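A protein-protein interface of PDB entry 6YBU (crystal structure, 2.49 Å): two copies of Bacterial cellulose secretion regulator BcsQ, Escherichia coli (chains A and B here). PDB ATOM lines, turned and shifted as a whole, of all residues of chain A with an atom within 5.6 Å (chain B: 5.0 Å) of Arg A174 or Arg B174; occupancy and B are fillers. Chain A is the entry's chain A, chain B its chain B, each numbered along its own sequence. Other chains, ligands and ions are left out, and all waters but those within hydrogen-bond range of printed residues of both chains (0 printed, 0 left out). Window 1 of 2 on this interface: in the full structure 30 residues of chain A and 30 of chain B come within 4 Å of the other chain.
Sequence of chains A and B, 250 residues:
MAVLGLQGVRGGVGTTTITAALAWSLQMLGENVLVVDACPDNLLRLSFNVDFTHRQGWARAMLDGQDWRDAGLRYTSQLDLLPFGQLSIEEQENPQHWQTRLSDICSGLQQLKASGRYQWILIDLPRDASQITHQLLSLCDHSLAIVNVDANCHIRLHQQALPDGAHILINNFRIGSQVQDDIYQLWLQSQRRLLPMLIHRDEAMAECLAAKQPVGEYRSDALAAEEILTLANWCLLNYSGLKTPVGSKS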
ATOM      1  N   ASN A 172     -15.010  21.441   0.047  1.00  0.00           N
ATOM      2  CA  ASN A 172     -14.287  21.764   1.278  1.00  0.00           C
ATOM      3  C   ASN A 172     -12.912  22.362   0.992  1.00  0.00           C
ATOM      4  O   ASN A 172     -11.981  22.220   1.788  1.00  0.00           O
ATOM      5  CB  ASN A 172     -14.161  20.537   2.187  1.00  0.00           C
ATOM      6  CG  ASN A 172     -14.244  20.891   3.658  1.00  0.00           C
ATOM      7  OD1 ASN A 172     -13.237  21.194   4.298  1.00  0.00           O
ATOM      8  ND2 ASN A 172     -15.453  20.855   4.203  1.00  0.00           N
ATOM      9  N   PHE A 173     -12.780  23.033  -0.151  1.00  0.00           N
ATOM     10  CA  PHE A 173     -11.531  23.692  -0.510  1.00  0.00           C
ATOM     11  C   PHE A 173     -11.194  24.762   0.523  1.00  0.00           C
ATOM     12  O   PHE A 173     -11.961  25.709   0.726  1.00  0.00           O
ATOM     13  CB  PHE A 173     -11.656  24.305  -1.904  1.00  0.00           C
ATOM     14  CG  PHE A 173     -10.340  24.618  -2.557  1.00  0.00           C
ATOM     15  CD1 PHE A 173      -9.536  23.600  -3.044  1.00  0.00           C
ATOM     16  CD2 PHE A 173      -9.920  25.929  -2.708  1.00  0.00           C
ATOM     17  CE1 PHE A 173      -8.328  23.881  -3.654  1.00  0.00           C
ATOM     18  CE2 PHE A 173      -8.711  26.219  -3.320  1.00  0.00           C
ATOM     19  CZ  PHE A 173      -7.914  25.191  -3.793  1.00  0.00           C
ATOM     20  N   ARG A 174     -10.052  24.606   1.183  1.00  0.00           N
ATOM     21  CA  ARG A 174      -9.660  25.480   2.277  1.00  0.00           C
ATOM     22  C   ARG A 174      -8.714  26.571   1.788  1.00  0.00           C
ATOM     23  O   ARG A 174      -8.128  26.485   0.705  1.00  0.00           O
ATOM     24  CB  ARG A 174      -9.001  24.676   3.400  1.00  0.00           C
ATOM     25  CG  ARG A 174      -9.889  23.583   3.974  1.00  0.00           C
ATOM     26  CD  ARG A 174      -9.206  22.848   5.111  1.00  0.00           C
ATOM     27  NE  ARG A 174     -10.049  21.782   5.650  1.00  0.00           N
ATOM     28  CZ  ARG A 174     -10.835  21.914   6.714  1.00  0.00           C
ATOM     29  NH1 ARG A 174     -10.888  23.068   7.365  1.00  0.00           N
ATOM     30  NH2 ARG A 174     -11.568  20.889   7.131  1.00  0.00           N
ATOM     31  N   ILE A 175      -8.582  27.615   2.605  1.00  0.00           N
ATOM     32  CA  ILE A 175      -7.692  28.738   2.332  1.00  0.00           C
ATOM     33  C   ILE A 175      -6.436  28.582   3.177  1.00  0.00           C
ATOM     34  O   ILE A 175      -6.511  28.265   4.372  1.00  0.00           O
ATOM     35  CB  ILE A 175      -8.388  30.084   2.615  1.00  0.00           C
ATOM     36  CG1 ILE A 175      -9.569  30.285   1.664  1.00  0.00           C
ATOM     37  CG2 ILE A 175      -7.403  31.243   2.499  1.00  0.00           C
ATOM     38  CD1 ILE A 175     -10.295  31.604   1.857  1.00  0.00           C
ATOM     39  N   GLY A 176      -5.279  28.789   2.556  1.00  0.00           N
ATOM     40  CA  GLY A 176      -4.027  28.774   3.287  1.00  0.00           C
ATOM     41  C   GLY A 176      -3.473  27.401   3.599  1.00  0.00           C
ATOM     42  O   GLY A 176      -2.909  27.197   4.681  1.00  0.00           O
ATOM     43  N   SER A 177      -3.618  26.448   2.681  1.00  0.00           N
ATOM     44  CA  SER A 177      -3.048  25.112   2.826  1.00  0.00           C
ATOM     45  C   SER A 177      -2.104  24.873   1.655  1.00  0.00           C
ATOM     46  O   SER A 177      -2.551  24.746   0.509  1.00  0.00           O
ATOM     47  CB  SER A 177      -4.140  24.044   2.879  1.00  0.00           C
ATOM     48  OG  SER A 177      -3.578  22.744   2.847  1.00  0.00           O
ATOM     49  N   GLN A 180      -2.547  21.510  -0.061  1.00  0.00           N
ATOM     50  CA  GLN A 180      -3.754  21.559  -0.879  1.00  0.00           C
ATOM     51  C   GLN A 180      -3.495  22.302  -2.182  1.00  0.00           C
ATOM     52  O   GLN A 180      -3.904  21.853  -3.260  1.00  0.00           O
ATOM     53  CB  GLN A 180      -4.896  22.221  -0.108  1.00  0.00           C
ATOM     54  CG  GLN A 180      -6.153  22.427  -0.943  1.00  0.00           C
ATOM     55  CD  GLN A 180      -7.140  23.383  -0.306  1.00  0.00           C
ATOM     56  OE1 GLN A 180      -8.021  22.974   0.452  1.00  0.00           O
ATOM     57  NE2 GLN A 180      -7.001  24.667  -0.616  1.00  0.00           N
ATOM     58  N   ASP A 181      -2.812  23.448  -2.099  1.00  0.00           N
ATOM     59  CA  ASP A 181      -2.495  24.214  -3.300  1.00  0.00           C
ATOM     60  C   ASP A 181      -1.650  23.398  -4.270  1.00  0.00           C
ATOM     61  O   ASP A 181      -1.848  23.469  -5.488  1.00  0.00           O
ATOM     62  CB  ASP A 181      -1.777  25.509  -2.921  1.00  0.00           C
ATOM     63  CG  ASP A 181      -2.653  26.448  -2.115  1.00  0.00           C
ATOM     64  OD1 ASP A 181      -3.830  26.105  -1.868  1.00  0.00           O
ATOM     65  OD2 ASP A 181      -2.162  27.531  -1.729  1.00  0.00           O
ATOM     66  N   HIS A 200     -15.896  25.821  -1.685  1.00  0.00           N
ATOM     67  CA  HIS A 200     -14.979  26.088  -0.591  1.00  0.00           C
ATOM     68  C   HIS A 200     -15.517  25.527   0.720  1.00  0.00           C
ATOM     69  O   HIS A 200     -16.710  25.245   0.870  1.00  0.00           O
ATOM     70  CB  HIS A 200     -14.745  27.591  -0.428  1.00  0.00           C
ATOM     71  CG  HIS A 200     -13.787  28.174  -1.418  1.00  0.00           C
ATOM     72  ND1 HIS A 200     -14.167  28.558  -2.685  1.00  0.00           N
ATOM     73  CD2 HIS A 200     -12.466  28.456  -1.320  1.00  0.00           C
ATOM     74  CE1 HIS A 200     -13.121  29.045  -3.328  1.00  0.00           C
ATOM     75  NE2 HIS A 200     -12.076  28.993  -2.523  1.00  0.00           N
ATOM     76  N   ARG A 201     -14.605  25.356   1.676  1.00  0.00           N
ATOM     77  CA  ARG A 201     -15.001  25.216   3.068  1.00  0.00           C
ATOM     78  C   ARG A 201     -15.824  26.432   3.476  1.00  0.00           C
ATOM     79  O   ARG A 201     -15.458  27.573   3.179  1.00  0.00           O
ATOM     80  CB  ARG A 201     -13.763  25.078   3.956  1.00  0.00           C
ATOM     81  CG  ARG A 201     -14.024  25.217   5.448  1.00  0.00           C
ATOM     82  CD  ARG A 201     -14.346  23.883   6.090  1.00  0.00           C
ATOM     83  NE  ARG A 201     -14.838  24.047   7.455  1.00  0.00           N
ATOM     84  CZ  ARG A 201     -15.362  23.068   8.185  1.00  0.00           C
ATOM     85  NH1 ARG A 201     -15.464  21.843   7.681  1.00  0.00           N
ATOM     86  NH2 ARG A 201     -15.790  23.313   9.416  1.00  0.00           N
ATOM     87  N   ASN B 148     -15.285  13.383  13.737  1.00  0.00           N
ATOM     88  CA  ASN B 148     -15.122  14.821  13.625  1.00  0.00           C
ATOM     89  C   ASN B 148     -16.291  15.487  14.337  1.00  0.00           C
ATOM     90  O   ASN B 148     -17.362  14.896  14.493  1.00  0.00           O
ATOM     91  CB  ASN B 148     -15.064  15.268  12.159  1.00  0.00           C
ATOM     92  CG  ASN B 148     -13.811  14.793  11.453  1.00  0.00           C
ATOM     93  OD1 ASN B 148     -12.970  14.109  12.042  1.00  0.00           O
ATOM     94  ND2 ASN B 148     -13.681  15.147  10.177  1.00  0.00           N
ATOM     95  N   VAL B 149     -16.078  16.722  14.787  1.00  0.00           N
ATOM     96  CA  VAL B 149     -17.122  17.465  15.493  1.00  0.00           C
ATOM     97  C   VAL B 149     -17.952  18.167  14.422  1.00  0.00           C
ATOM     98  O   VAL B 149     -17.703  19.316  14.059  1.00  0.00           O
ATOM     99  CB  VAL B 149     -16.549  18.435  16.520  1.00  0.00           C
ATOM    100  CG1 VAL B 149     -17.673  19.040  17.352  1.00  0.00           C
ATOM    101  CG2 VAL B 149     -15.556  17.726  17.415  1.00  0.00           C
ATOM    102  N   ASN B 172      -9.616  16.509  13.806  1.00  0.00           N
ATOM    103  CA  ASN B 172      -9.881  17.656  12.936  1.00  0.00           C
ATOM    104  C   ASN B 172     -10.586  18.796  13.665  1.00  0.00           C
ATOM    105  O   ASN B 172     -11.365  19.535  13.060  1.00  0.00           O
ATOM    106  CB  ASN B 172     -10.692  17.251  11.700  1.00  0.00           C
ATOM    107  CG  ASN B 172      -9.832  17.087  10.465  1.00  0.00           C
ATOM    108  OD1 ASN B 172      -9.384  18.069   9.872  1.00  0.00           O
ATOM    109  ND2 ASN B 172      -9.605  15.841  10.064  1.00  0.00           N
ATOM    110  N   PHE B 173     -10.323  18.959  14.960  1.00  0.00           N
ATOM    111  CA  PHE B 173     -10.930  20.051  15.708  1.00  0.00           C
ATOM    112  C   PHE B 173     -10.421  21.389  15.181  1.00  0.00           C
ATOM    113  O   PHE B 173      -9.211  21.633  15.147  1.00  0.00           O
ATOM    114  CB  PHE B 173     -10.624  19.904  17.196  1.00  0.00           C
ATOM    115  CG  PHE B 173     -11.587  20.633  18.086  1.00  0.00           C
ATOM    116  CD1 PHE B 173     -12.877  20.154  18.268  1.00  0.00           C
ATOM    117  CD2 PHE B 173     -11.207  21.791  18.746  1.00  0.00           C
ATOM    118  CE1 PHE B 173     -13.771  20.818  19.088  1.00  0.00           C
ATOM    119  CE2 PHE B 173     -12.097  22.459  19.569  1.00  0.00           C
ATOM    120  CZ  PHE B 173     -13.382  21.971  19.741  1.00  0.00           C
ATOM    121  N   ARG B 174     -11.346  22.251  14.769  1.00  0.00           N
ATOM    122  CA  ARG B 174     -11.011  23.480  14.066  1.00  0.00           C
ATOM    123  C   ARG B 174     -11.129  24.689  14.988  1.00  0.00           C
ATOM    124  O   ARG B 174     -11.704  24.627  16.076  1.00  0.00           O
ATOM    125  CB  ARG B 174     -11.909  23.650  12.838  1.00  0.00           C
ATOM    126  CG  ARG B 174     -11.768  22.522  11.832  1.00  0.00           C
ATOM    127  CD  ARG B 174     -12.879  22.537  10.800  1.00  0.00           C
ATOM    128  NE  ARG B 174     -12.803  21.369   9.925  1.00  0.00           N
ATOM    129  CZ  ARG B 174     -13.402  20.208  10.173  1.00  0.00           C
ATOM    130  NH1 ARG B 174     -14.131  20.059  11.270  1.00  0.00           N
ATOM    131  NH2 ARG B 174     -13.275  19.197   9.324  1.00  0.00           N
ATOM    132  N   ILE B 175     -10.566  25.803  14.530  1.00  0.00           N
ATOM    133  CA  ILE B 175     -10.566  27.060  15.271  1.00  0.00           C
ATOM    134  C   ILE B 175     -11.583  27.998  14.640  1.00  0.00           C
ATOM    135  O   ILE B 175     -11.565  28.218  13.423  1.00  0.00           O
ATOM    136  CB  ILE B 175      -9.167  27.701  15.282  1.00  0.00           C
ATOM    137  CG1 ILE B 175      -8.165  26.784  15.988  1.00  0.00           C
ATOM    138  CG2 ILE B 175      -9.210  29.074  15.945  1.00  0.00           C
ATOM    139  CD1 ILE B 175      -8.548  26.444  17.413  1.00  0.00           C
ATOM    140  N   GLY B 176     -12.476  28.543  15.461  1.00  0.00           N
ATOM    141  CA  GLY B 176     -13.404  29.553  14.990  1.00  0.00           C
ATOM    142  C   GLY B 176     -14.638  29.032  14.291  1.00  0.00           C
ATOM    143  O   GLY B 176     -15.122  29.669  13.349  1.00  0.00           O
ATOM    144  N   SER B 177     -15.164  27.887  14.717  1.00  0.00           N
ATOM    145  CA  SER B 177     -16.414  27.349  14.192  1.00  0.00           C
ATOM    146  C   SER B 177     -17.435  27.348  15.321  1.00  0.00           C
ATOM    147  O   SER B 177     -17.316  26.567  16.272  1.00  0.00           O
ATOM    148  CB  SER B 177     -16.220  25.947  13.619  1.00  0.00           C
ATOM    149  OG  SER B 177     -17.463  25.384  13.232  1.00  0.00           O
ATOM    150  N   GLN B 180     -19.269  24.065  15.669  1.00  0.00           N
ATOM    151  CA  GLN B 180     -18.407  23.057  16.278  1.00  0.00           C
ATOM    152  C   GLN B 180     -18.335  23.241  17.786  1.00  0.00           C
ATOM    153  O   GLN B 180     -18.388  22.263  18.540  1.00  0.00           O
ATOM    154  CB  GLN B 180     -17.007  23.113  15.672  1.00  0.00           C
ATOM    155  CG  GLN B 180     -16.076  22.034  16.203  1.00  0.00           C
ATOM    156  CD  GLN B 180     -14.612  22.371  16.011  1.00  0.00           C
ATOM    157  OE1 GLN B 180     -13.939  21.805  15.148  1.00  0.00           O
ATOM    158  NE2 GLN B 180     -14.107  23.293  16.824  1.00  0.00           N
ATOM    159  N   ARG B 201      -7.248  20.101  13.875  1.00  0.00           N
ATOM    160  CA  ARG B 201      -6.866  20.125  12.470  1.00  0.00           C
ATOM    161  C   ARG B 201      -5.488  20.758  12.346  1.00  0.00           C
ATOM    162  O   ARG B 201      -5.284  21.904  12.759  1.00  0.00           O
ATOM    163  CB  ARG B 201      -7.882  20.893  11.629  1.00  0.00           C
ATOM    164  CG  ARG B 201      -7.268  21.403  10.331  1.00  0.00           C
ATOM    165  CD  ARG B 201      -8.252  21.549   9.195  1.00  0.00           C
ATOM    166  NE  ARG B 201      -7.531  21.672   7.931  1.00  0.00           N
ATOM    167  CZ  ARG B 201      -7.377  20.682   7.057  1.00  0.00           C
ATOM    168  NH1 ARG B 201      -7.912  19.493   7.298  1.00  0.00           N
ATOM    169  NH2 ARG B 201      -6.699  20.886   5.937  1.00  0.00           N
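Arg B174 touches Arg A201 (CD to NH2, 3.3 Å).
The backbone carbonyl oxygen (O) of Phe A173 is in hydrogen-bond range of the backbone NH (N) of Arg A201, 2.8 Å away.
O of Arg A174 lies within hydrogen-bond range of NE2 of Gln A180, 2.5 Å away.
The guanidinium group (NH1) of Arg B174 sits close to the backbone carbonyl oxygen (O) of Asn B172 (3.3 Å).
OD1 of Asn B172 is in hydrogen-bond range of NH1 of Arg B201 (3.3 Å).
O of Phe B173 is in hydrogen-bond range of N of Arg B201, 2.8 Å away.
The backbone NH of Arg B174 sits at hydrogen-bond distance from the side-chain amide oxygen of Gln B180.
The guanidinium group (NH2) of Arg A174 sits close to the guanidinium group (NE) of Arg B174 (3.1 Å).
NE of Arg A174 lies close to NE of Arg B201 (3.4 Å).
Of chain B, only Arg B174 (3.1 Å) and Arg B201 (3.2 Å) come within 4 Å of Arg A174.
Gly A176 touches none of the printed residues of chain B.
Printed residues of chain B within 4 Å of Arg A201: Arg B174 (3.3 Å).
Printed residues of chain A within 4 Å of Arg B174: Arg A174 and Arg A201.
Of the printed residues of chain A, Arg B201 touches Arg A174 (3.2 Å).
The nearest residue of chain B that does not touch Arg A174 is Asn B172 (4.5 Å).
The nearest residue of chain A that does not touch Arg B174 is Asn A172 (5.4 Å).
Arg A174 touches its own counterpart, Arg B174.
Arg A174 touches Arg B201, and with the chains exchanged Arg A201 touches Arg B174.
8 positions are printed for both chains.
Of the 3 pairs that touch across the chains among the printed residues, 3 have their exchanged pair printed and touching as well.
Of the 10 printed residues of chain A, 2 touch a printed residue of chain B.
Among the printed residues, no Asp or Glu carboxylate lies within 4 Å of a Lys or Arg side-chain nitrogen of the other chain.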
